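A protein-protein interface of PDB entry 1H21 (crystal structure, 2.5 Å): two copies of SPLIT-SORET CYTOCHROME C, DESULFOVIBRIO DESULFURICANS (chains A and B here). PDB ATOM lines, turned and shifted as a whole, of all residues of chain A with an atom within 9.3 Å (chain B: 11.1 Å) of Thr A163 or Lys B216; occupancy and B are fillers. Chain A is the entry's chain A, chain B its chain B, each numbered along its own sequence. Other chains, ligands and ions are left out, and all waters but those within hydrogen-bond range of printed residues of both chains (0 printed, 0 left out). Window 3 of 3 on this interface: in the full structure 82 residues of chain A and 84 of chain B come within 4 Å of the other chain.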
ATOM      1  N   VAL A 133     -20.305  27.113 -15.253  1.00  0.00           N
ATOM      2  CA  VAL A 133     -21.294  27.223 -16.320  1.00  0.00           C
ATOM      3  C   VAL A 133     -20.811  28.293 -17.308  1.00  0.00           C
ATOM      4  O   VAL A 133     -20.360  29.381 -16.907  1.00  0.00           O
ATOM      5  CB  VAL A 133     -22.702  27.593 -15.805  1.00  0.00           C
ATOM      6  CG1 VAL A 133     -23.163  26.612 -14.768  1.00  0.00           C
ATOM      7  CG2 VAL A 133     -22.746  29.041 -15.294  1.00  0.00           C
ATOM      8  N   VAL A 151     -24.306  37.326  -1.625  1.00  0.00           N
ATOM      9  CA  VAL A 151     -24.859  36.140  -2.272  1.00  0.00           C
ATOM     10  C   VAL A 151     -26.382  35.974  -2.129  1.00  0.00           C
ATOM     11  O   VAL A 151     -27.087  35.873  -3.131  1.00  0.00           O
ATOM     12  CB  VAL A 151     -24.125  34.841  -1.806  1.00  0.00           C
ATOM     13  CG1 VAL A 151     -24.743  33.614  -2.470  1.00  0.00           C
ATOM     14  CG2 VAL A 151     -22.622  34.922  -2.137  1.00  0.00           C
ATOM     15  N   TRP A 154     -28.516  38.461  -4.268  1.00  0.00           N
ATOM     16  CA  TRP A 154     -28.408  38.125  -5.684  1.00  0.00           C
ATOM     17  C   TRP A 154     -29.239  36.879  -6.065  1.00  0.00           C
ATOM     18  O   TRP A 154     -29.959  36.898  -7.065  1.00  0.00           O
ATOM     19  CB  TRP A 154     -26.927  37.933  -6.034  1.00  0.00           C
ATOM     20  CG  TRP A 154     -26.625  37.583  -7.467  1.00  0.00           C
ATOM     21  CD1 TRP A 154     -26.332  38.454  -8.488  1.00  0.00           C
ATOM     22  CD2 TRP A 154     -26.486  36.264  -8.017  1.00  0.00           C
ATOM     23  NE1 TRP A 154     -26.008  37.755  -9.624  1.00  0.00           N
ATOM     24  CE2 TRP A 154     -26.092  36.411  -9.365  1.00  0.00           C
ATOM     25  CE3 TRP A 154     -26.645  34.968  -7.490  1.00  0.00           C
ATOM     26  CZ2 TRP A 154     -25.852  35.311 -10.203  1.00  0.00           C
ATOM     27  CZ3 TRP A 154     -26.406  33.877  -8.318  1.00  0.00           C
ATOM     28  CH2 TRP A 154     -26.012  34.055  -9.664  1.00  0.00           C
ATOM     29  N   CYS A 155     -29.128  35.799  -5.289  1.00  0.00           N
ATOM     30  CA  CYS A 155     -29.886  34.569  -5.550  1.00  0.00           C
ATOM     31  C   CYS A 155     -31.392  34.838  -5.461  1.00  0.00           C
ATOM     32  O   CYS A 155     -32.174  34.417  -6.325  1.00  0.00           O
ATOM     33  CB  CYS A 155     -29.493  33.453  -4.564  1.00  0.00           C
ATOM     34  SG  CYS A 155     -27.911  32.598  -4.894  1.00  0.00           S
ATOM     35  N   ILE A 160     -32.347  32.215  -8.345  1.00  0.00           N
ATOM     36  CA  ILE A 160     -31.338  31.176  -8.538  1.00  0.00           C
ATOM     37  C   ILE A 160     -31.053  30.600  -7.154  1.00  0.00           C
ATOM     38  O   ILE A 160     -31.093  31.322  -6.152  1.00  0.00           O
ATOM     39  CB  ILE A 160     -30.015  31.763  -9.103  1.00  0.00           C
ATOM     40  CG1 ILE A 160     -30.258  32.361 -10.480  1.00  0.00           C
ATOM     41  CG2 ILE A 160     -28.942  30.685  -9.206  1.00  0.00           C
ATOM     42  CD1 ILE A 160     -29.203  33.336 -10.887  1.00  0.00           C
ATOM     43  N   GLU A 161     -30.798  29.299  -7.090  1.00  0.00           N
ATOM     44  CA  GLU A 161     -30.495  28.659  -5.816  1.00  0.00           C
ATOM     45  C   GLU A 161     -29.029  28.872  -5.447  1.00  0.00           C
ATOM     46  O   GLU A 161     -28.145  28.795  -6.313  1.00  0.00           O
ATOM     47  CB  GLU A 161     -30.810  27.157  -5.870  1.00  0.00           C
ATOM     48  CG  GLU A 161     -32.271  26.790  -5.612  1.00  0.00           C
ATOM     49  CD  GLU A 161     -32.467  25.281  -5.427  1.00  0.00           C
ATOM     50  OE1 GLU A 161     -31.948  24.713  -4.437  1.00  0.00           O
ATOM     51  OE2 GLU A 161     -33.141  24.651  -6.275  1.00  0.00           O
ATOM     52  N   ALA A 162     -28.767  29.087  -4.159  1.00  0.00           N
ATOM     53  CA  ALA A 162     -27.406  29.309  -3.656  1.00  0.00           C
ATOM     54  C   ALA A 162     -26.528  28.048  -3.799  1.00  0.00           C
ATOM     55  O   ALA A 162     -25.328  28.037  -3.476  1.00  0.00           O
ATOM     56  CB  ALA A 162     -27.469  29.765  -2.209  1.00  0.00           C
ATOM     57  N   THR A 163     -27.149  27.001  -4.322  1.00  0.00           N
ATOM     58  CA  THR A 163     -26.557  25.692  -4.556  1.00  0.00           C
ATOM     59  C   THR A 163     -26.246  25.526  -6.058  1.00  0.00           C
ATOM     60  O   THR A 163     -25.476  24.649  -6.449  1.00  0.00           O
ATOM     61  CB  THR A 163     -27.615  24.619  -4.085  1.00  0.00           C
ATOM     62  OG1 THR A 163     -27.032  23.752  -3.109  1.00  0.00           O
ATOM     63  CG2 THR A 163     -28.232  23.817  -5.278  1.00  0.00           C
ATOM     64  N   SER A 164     -26.883  26.354  -6.886  1.00  0.00           N
ATOM     65  CA  SER A 164     -26.742  26.304  -8.340  1.00  0.00           C
ATOM     66  C   SER A 164     -25.314  26.437  -8.812  1.00  0.00           C
ATOM     67  O   SER A 164     -24.486  27.073  -8.144  1.00  0.00           O
ATOM     68  CB  SER A 164     -27.582  27.422  -8.976  1.00  0.00           C
ATOM     69  OG  SER A 164     -27.626  27.303 -10.388  1.00  0.00           O
ATOM     70  N   LYS A 165     -25.046  25.876  -9.995  1.00  0.00           N
ATOM     71  CA  LYS A 165     -23.711  25.957 -10.601  1.00  0.00           C
ATOM     72  C   LYS A 165     -23.439  27.405 -10.966  1.00  0.00           C
ATOM     73  O   LYS A 165     -22.289  27.841 -11.062  1.00  0.00           O
ATOM     74  CB  LYS A 165     -23.629  25.091 -11.852  1.00  0.00           C
ATOM     75  CG  LYS A 165     -23.394  23.630 -11.556  1.00  0.00           C
ATOM     76  CD  LYS A 165     -22.570  22.989 -12.664  1.00  0.00           C
ATOM     77  CE  LYS A 165     -22.246  21.537 -12.341  1.00  0.00           C
ATOM     78  NZ  LYS A 165     -21.178  21.003 -13.232  1.00  0.00           N
ATOM     79  N   GLN A 166     -24.518  28.148 -11.159  1.00  0.00           N
ATOM     80  CA  GLN A 166     -24.431  29.551 -11.502  1.00  0.00           C
ATOM     81  C   GLN A 166     -23.844  30.396 -10.408  1.00  0.00           C
ATOM     82  O   GLN A 166     -22.996  31.228 -10.672  1.00  0.00           O
ATOM     83  CB  GLN A 166     -25.814  30.099 -11.846  1.00  0.00           C
ATOM     84  CG  GLN A 166     -26.322  29.805 -13.235  1.00  0.00           C
ATOM     85  CD  GLN A 166     -27.803  29.706 -13.227  1.00  0.00           C
ATOM     86  OE1 GLN A 166     -28.357  28.738 -12.691  1.00  0.00           O
ATOM     87  NE2 GLN A 166     -28.477  30.729 -13.738  1.00  0.00           N
ATOM     88  N   ARG A 167     -24.292  30.201  -9.175  1.00  0.00           N
ATOM     89  CA  ARG A 167     -23.767  31.046  -8.120  1.00  0.00           C
ATOM     90  C   ARG A 167     -22.323  30.704  -7.774  1.00  0.00           C
ATOM     91  O   ARG A 167     -21.563  31.574  -7.330  1.00  0.00           O
ATOM     92  CB  ARG A 167     -24.717  31.142  -6.911  1.00  0.00           C
ATOM     93  CG  ARG A 167     -24.516  30.144  -5.827  1.00  0.00           C
ATOM     94  CD  ARG A 167     -23.564  30.626  -4.736  1.00  0.00           C
ATOM     95  NE  ARG A 167     -22.763  29.485  -4.298  1.00  0.00           N
ATOM     96  CZ  ARG A 167     -21.468  29.533  -4.006  1.00  0.00           C
ATOM     97  NH1 ARG A 167     -20.804  30.688  -4.067  1.00  0.00           N
ATOM     98  NH2 ARG A 167     -20.809  28.406  -3.796  1.00  0.00           N
ATOM     99  N   SER A 168     -21.923  29.457  -8.002  1.00  0.00           N
ATOM    100  CA  SER A 168     -20.542  29.090  -7.751  1.00  0.00           C
ATOM    101  C   SER A 168     -19.708  29.636  -8.926  1.00  0.00           C
ATOM    102  O   SER A 168     -18.530  29.935  -8.771  1.00  0.00           O
ATOM    103  CB  SER A 168     -20.384  27.581  -7.607  1.00  0.00           C
ATOM    104  OG  SER A 168     -20.478  26.925  -8.852  1.00  0.00           O
ATOM    105  N   GLU A 169     -20.331  29.766 -10.100  1.00  0.00           N
ATOM    106  CA  GLU A 169     -19.653  30.331 -11.262  1.00  0.00           C
ATOM    107  C   GLU A 169     -19.512  31.816 -10.949  1.00  0.00           C
ATOM    108  O   GLU A 169     -18.447  32.400 -11.117  1.00  0.00           O
ATOM    109  CB  GLU A 169     -20.495  30.137 -12.528  1.00  0.00           C
ATOM    110  CG  GLU A 169     -19.903  30.757 -13.803  1.00  0.00           C
ATOM    111  CD  GLU A 169     -18.577  30.137 -14.243  1.00  0.00           C
ATOM    112  OE1 GLU A 169     -18.424  28.904 -14.185  1.00  0.00           O
ATOM    113  OE2 GLU A 169     -17.688  30.897 -14.688  1.00  0.00           O
ATOM    114  N   SER B 207     -31.106  26.328  11.802  1.00  0.00           N
ATOM    115  CA  SER B 207     -31.709  25.117  11.261  1.00  0.00           C
ATOM    116  C   SER B 207     -33.201  25.319  10.998  1.00  0.00           C
ATOM    117  O   SER B 207     -33.703  24.813   9.996  1.00  0.00           O
ATOM    118  CB  SER B 207     -31.405  23.858  12.094  1.00  0.00           C
ATOM    119  OG  SER B 207     -31.659  24.078  13.460  1.00  0.00           O
ATOM    120  N   CYS B 209     -34.806  28.330  10.183  1.00  0.00           N
ATOM    121  CA  CYS B 209     -34.862  29.146   8.952  1.00  0.00           C
ATOM    122  C   CYS B 209     -34.212  28.373   7.790  1.00  0.00           C
ATOM    123  O   CYS B 209     -34.660  28.453   6.635  1.00  0.00           O
ATOM    124  CB  CYS B 209     -34.098  30.445   9.111  1.00  0.00           C
ATOM    125  SG  CYS B 209     -34.603  31.469  10.469  1.00  0.00           S
ATOM    126  N   GLY B 210     -33.137  27.656   8.105  1.00  0.00           N
ATOM    127  CA  GLY B 210     -32.429  26.861   7.129  1.00  0.00           C
ATOM    128  C   GLY B 210     -33.284  25.802   6.485  1.00  0.00           C
ATOM    129  O   GLY B 210     -33.023  25.442   5.342  1.00  0.00           O
ATOM    130  N   GLU B 211     -34.307  25.315   7.181  1.00  0.00           N
ATOM    131  CA  GLU B 211     -35.185  24.292   6.611  1.00  0.00           C
ATOM    132  C   GLU B 211     -35.660  24.711   5.223  1.00  0.00           C
ATOM    133  O   GLU B 211     -35.834  23.886   4.337  1.00  0.00           O
ATOM    134  CB  GLU B 211     -36.413  24.052   7.488  1.00  0.00           C
ATOM    135  N   CYS B 212     -35.858  26.003   5.035  1.00  0.00           N
ATOM    136  CA  CYS B 212     -36.307  26.532   3.761  1.00  0.00           C
ATOM    137  C   CYS B 212     -35.214  27.222   2.941  1.00  0.00           C
ATOM    138  O   CYS B 212     -35.095  27.019   1.728  1.00  0.00           O
ATOM    139  CB  CYS B 212     -37.400  27.560   4.013  1.00  0.00           C
ATOM    140  SG  CYS B 212     -39.028  26.901   4.401  1.00  0.00           S
ATOM    141  N   HIS B 213     -34.433  28.050   3.628  1.00  0.00           N
ATOM    142  CA  HIS B 213     -33.400  28.865   3.018  1.00  0.00           C
ATOM    143  C   HIS B 213     -32.054  28.295   2.681  1.00  0.00           C
ATOM    144  O   HIS B 213     -31.342  28.860   1.851  1.00  0.00           O
ATOM    145  CB  HIS B 213     -33.246  30.136   3.828  1.00  0.00           C
ATOM    146  CG  HIS B 213     -34.439  31.026   3.726  1.00  0.00           C
ATOM    147  ND1 HIS B 213     -34.992  31.429   2.530  1.00  0.00           N
ATOM    148  CD2 HIS B 213     -35.235  31.547   4.689  1.00  0.00           C
ATOM    149  CE1 HIS B 213     -36.074  32.153   2.793  1.00  0.00           C
ATOM    150  NE2 HIS B 213     -36.269  32.256   4.090  1.00  0.00           N
ATOM    151  N   MET B 214     -31.683  27.207   3.337  1.00  0.00           N
ATOM    152  CA  MET B 214     -30.398  26.583   3.071  1.00  0.00           C
ATOM    153  C   MET B 214     -30.566  25.101   2.838  1.00  0.00           C
ATOM    154  O   MET B 214     -29.793  24.301   3.351  1.00  0.00           O
ATOM    155  CB  MET B 214     -29.434  26.800   4.238  1.00  0.00           C
ATOM    156  CG  MET B 214     -28.895  28.209   4.367  1.00  0.00           C
ATOM    157  SD  MET B 214     -29.515  28.966   5.845  1.00  0.00           S
ATOM    158  CE  MET B 214     -29.694  30.528   5.379  1.00  0.00           C
ATOM    159  N   THR B 215     -31.581  24.736   2.069  1.00  0.00           N
ATOM    160  CA  THR B 215     -31.862  23.335   1.771  1.00  0.00           C
ATOM    161  C   THR B 215     -32.087  23.181   0.265  1.00  0.00           C
ATOM    162  O   THR B 215     -32.968  23.818  -0.318  1.00  0.00           O
ATOM    163  CB  THR B 215     -33.090  22.822   2.568  1.00  0.00           C
ATOM    164  OG1 THR B 215     -32.926  23.150   3.955  1.00  0.00           O
ATOM    165  CG2 THR B 215     -33.209  21.308   2.443  1.00  0.00           C
ATOM    166  N   LYS B 216     -31.246  22.354  -0.351  1.00  0.00           N
ATOM    167  CA  LYS B 216     -31.264  22.108  -1.789  1.00  0.00           C
ATOM    168  C   LYS B 216     -32.665  21.707  -2.300  1.00  0.00           C
ATOM    169  O   LYS B 216     -33.376  20.950  -1.630  1.00  0.00           O
ATOM    170  CB  LYS B 216     -30.209  21.030  -2.109  1.00  0.00           C
ATOM    171  CG  LYS B 216     -29.845  20.889  -3.582  1.00  0.00           C
ATOM    172  CD  LYS B 216     -28.643  19.962  -3.804  1.00  0.00           C
ATOM    173  CE  LYS B 216     -28.045  20.235  -5.174  1.00  0.00           C
ATOM    174  NZ  LYS B 216     -27.712  19.053  -5.975  1.00  0.00           N
ATOM    175  N   GLY B 217     -33.097  22.259  -3.431  1.00  0.00           N
ATOM    176  CA  GLY B 217     -34.399  21.888  -3.963  1.00  0.00           C
ATOM    177  C   GLY B 217     -35.582  22.753  -3.577  1.00  0.00           C
ATOM    178  O   GLY B 217     -36.587  22.777  -4.287  1.00  0.00           O
ATOM    179  N   ASN B 218     -35.499  23.413  -2.432  1.00  0.00           N
ATOM    180  CA  ASN B 218     -36.553  24.313  -1.956  1.00  0.00           C
ATOM    181  C   ASN B 218     -36.485  25.619  -2.767  1.00  0.00           C
ATOM    182  O   ASN B 218     -35.395  26.152  -2.995  1.00  0.00           O
ATOM    183  CB  ASN B 218     -36.289  24.630  -0.470  1.00  0.00           C
ATOM    184  CG  ASN B 218     -37.470  25.270   0.224  1.00  0.00           C
ATOM    185  OD1 ASN B 218     -37.987  26.317  -0.199  1.00  0.00           O
ATOM    186  ND2 ASN B 218     -37.892  24.656   1.321  1.00  0.00           N
ATOM    187  N   ASP B 219     -37.635  26.134  -3.191  1.00  0.00           N
ATOM    188  CA  ASP B 219     -37.729  27.397  -3.951  1.00  0.00           C
ATOM    189  C   ASP B 219     -36.992  28.551  -3.267  1.00  0.00           C
ATOM    190  O   ASP B 219     -36.418  29.435  -3.916  1.00  0.00           O
ATOM    191  CB  ASP B 219     -39.185  27.874  -3.963  1.00  0.00           C
ATOM    192  CG  ASP B 219     -40.017  27.275  -5.043  1.00  0.00           C
ATOM    193  OD1 ASP B 219     -40.248  26.047  -5.058  1.00  0.00           O
ATOM    194  OD2 ASP B 219     -40.522  28.080  -5.843  1.00  0.00           O
ATOM    195  N   ALA B 220     -37.150  28.596  -1.949  1.00  0.00           N
ATOM    196  CA  ALA B 220     -36.583  29.642  -1.118  1.00  0.00           C
ATOM    197  C   ALA B 220     -35.111  29.452  -0.763  1.00  0.00           C
ATOM    198  O   ALA B 220     -34.580  30.206   0.063  1.00  0.00           O
ATOM    199  CB  ALA B 220     -37.419  29.797   0.153  1.00  0.00           C
ATOM    200  N   ASN B 221     -34.455  28.464  -1.380  1.00  0.00           N
ATOM    201  CA  ASN B 221     -33.030  28.180  -1.119  1.00  0.00           C
ATOM    202  C   ASN B 221     -32.078  29.224  -1.747  1.00  0.00           C
ATOM    203  O   ASN B 221     -31.359  28.957  -2.724  1.00  0.00           O
ATOM    204  CB  ASN B 221     -32.676  26.764  -1.589  1.00  0.00           C
ATOM    205  CG  ASN B 221     -31.247  26.398  -1.286  1.00  0.00           C
ATOM    206  OD1 ASN B 221     -30.746  26.651  -0.184  1.00  0.00           O
ATOM    207  ND2 ASN B 221     -30.557  25.832  -2.277  1.00  0.00           N
ATOM    208  N   TRP B 222     -32.052  30.404  -1.135  1.00  0.00           N
ATOM    209  CA  TRP B 222     -31.236  31.510  -1.607  1.00  0.00           C
ATOM    210  C   TRP B 222     -30.099  31.937  -0.685  1.00  0.00           C
ATOM    211  O   TRP B 222     -29.137  32.539  -1.153  1.00  0.00           O
ATOM    212  CB  TRP B 222     -32.114  32.734  -1.821  1.00  0.00           C
ATOM    213  CG  TRP B 222     -33.312  32.506  -2.658  1.00  0.00           C
ATOM    214  CD1 TRP B 222     -33.354  31.991  -3.925  1.00  0.00           C
ATOM    215  CD2 TRP B 222     -34.648  32.859  -2.321  1.00  0.00           C
ATOM    216  NE1 TRP B 222     -34.638  32.016  -4.402  1.00  0.00           N
ATOM    217  CE2 TRP B 222     -35.457  32.544  -3.438  1.00  0.00           C
ATOM    218  CE3 TRP B 222     -35.249  33.415  -1.182  1.00  0.00           C
ATOM    219  CZ2 TRP B 222     -36.843  32.767  -3.450  1.00  0.00           C
ATOM    220  CZ3 TRP B 222     -36.625  33.638  -1.190  1.00  0.00           C
ATOM    221  CH2 TRP B 222     -37.407  33.311  -2.322  1.00  0.00           C
ATOM    222  N   ALA B 223     -30.186  31.615   0.605  1.00  0.00           N
ATOM    223  CA  ALA B 223     -29.174  32.083   1.543  1.00  0.00           C
ATOM    224  C   ALA B 223     -27.900  31.276   1.700  1.00  0.00           C
ATOM    225  O   ALA B 223     -27.869  30.072   1.434  1.00  0.00           O
ATOM    226  CB  ALA B 223     -29.803  32.368   2.884  1.00  0.00           C
ATOM    227  N   LYS B 224     -26.835  31.979   2.088  1.00  0.00           N
ATOM    228  CA  LYS B 224     -25.511  31.382   2.311  1.00  0.00           C
ATOM    229  C   LYS B 224     -25.012  32.003   3.594  1.00  0.00           C
ATOM    230  O   LYS B 224     -25.041  33.217   3.747  1.00  0.00           O
ATOM    231  CB  LYS B 224     -24.556  31.756   1.179  1.00  0.00           C
ATOM    232  CG  LYS B 224     -23.682  30.632   0.655  1.00  0.00           C
ATOM    233  CD  LYS B 224     -24.477  29.354   0.285  1.00  0.00           C
ATOM    234  CE  LYS B 224     -23.640  28.376  -0.584  1.00  0.00           C
ATOM    235  NZ  LYS B 224     -24.233  27.008  -0.738  1.00  0.00           N
ATOM    236  N   GLY B 225     -24.594  31.178   4.534  1.00  0.00           N
ATOM    237  CA  GLY B 225     -24.138  31.711   5.800  1.00  0.00           C
ATOM    238  C   GLY B 225     -24.818  31.003   6.953  1.00  0.00           C
ATOM    239  O   GLY B 225     -26.019  30.730   6.911  1.00  0.00           O
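Hydrophobic or aromatic side chains of chain B within 4 Å of the printed part of chain A: Trp B222. Of the 14 printed residues of chain A, 6 touch a printed residue of chain B. Printed residues of chain A that touch a printed residue of chain B: Cys A155, Ile A160, Glu A161, Ala A162, Thr A163 and Arg A167. Hydrophobic or aromatic side chains of chain A within 4 Å of the printed part of chain B: Ala A162. Among the printed residues, 13 pairs touch across the chains.
Cys A155 touches Trp B222. O of Ile A160 touches CD1 of Trp B222, 3.2 Å away. Glu A161 touches Lys B216. Asn B218 touches Glu A161 (O to CD, 3.9 Å). O of Trp B222 touches CB of Ala A162, 3.4 Å away. Ala A162 touches Ala B223. Thr A163 touches Lys B216. ND2 of Asn B221 touches CB of Thr A163, 3.7 Å away. Arg A167 touches Lys B224 (NE to CE, 3.97 Å).
No position is printed for both chains.
Thr A163 touches just these residues of chain B: Lys B216 and Asn B221. Of chain A, only Glu A161 and Thr A163 come within 4 Å of Lys B216. Printed residues of chain B within 4 Å of Glu A161: Lys B216 (3.8 Å), Gly B217 (2.9 Å), Asn B218 (3.9 Å) and Asn B221 (2.8 Å). Of chain B, only Asn B221 (3.0 Å), Trp B222 (3.4 Å), Ala B223 (3.7 Å) and Lys B224 (3.1 Å) come within 4 Å of Ala A162. No residue of chain B comes within 4 Å of Ser A164. No residue of chain A comes within 4 Å of Thr B215. Printed residues of chain B within 4 Å of Ile A160: Trp B222 (3.2 Å). Of the printed residues of chain A, Lys B224 touches Ala A162 and Arg A167. The nearest residue of chain B that does not touch Thr A163 is Lys B224 (4.6 Å).
The backbone NH of Asn B221 is in hydrogen-bond range of the backbone carbonyl oxygen of Cys B212 (3.5 Å). OD1 of Asn B221 sits close to O of His B213 (3.1 Å). The backbone NH (N) of Trp B222 lies within hydrogen-bond range of the backbone carbonyl oxygen (O) of His B213 (3.4 Å). The side-chain amide oxygen (OD1) of Asn B221 is in hydrogen-bond range of the backbone NH (N) of Thr B215 (3.1 Å). OD1 of Asn B218 sits at hydrogen-bond distance from N of Ala B220 (3.0 Å). NE1 of Trp B222 lies within hydrogen-bond range of O of Asp B219 (3.2 Å).
N of Gly B217 lies within hydrogen-bond range of OE1 of Glu A161, 2.9 Å away. OE1 of Glu A161 sits at hydrogen-bond distance from ND2 of Asn B221 (2.8 Å). The backbone carbonyl oxygen of Asn B221 lies within hydrogen-bond range of the backbone NH of Ala A162 (3.0 Å). O of Ala A162 lies within hydrogen-bond range of NZ of Lys B224 (3.1 Å).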
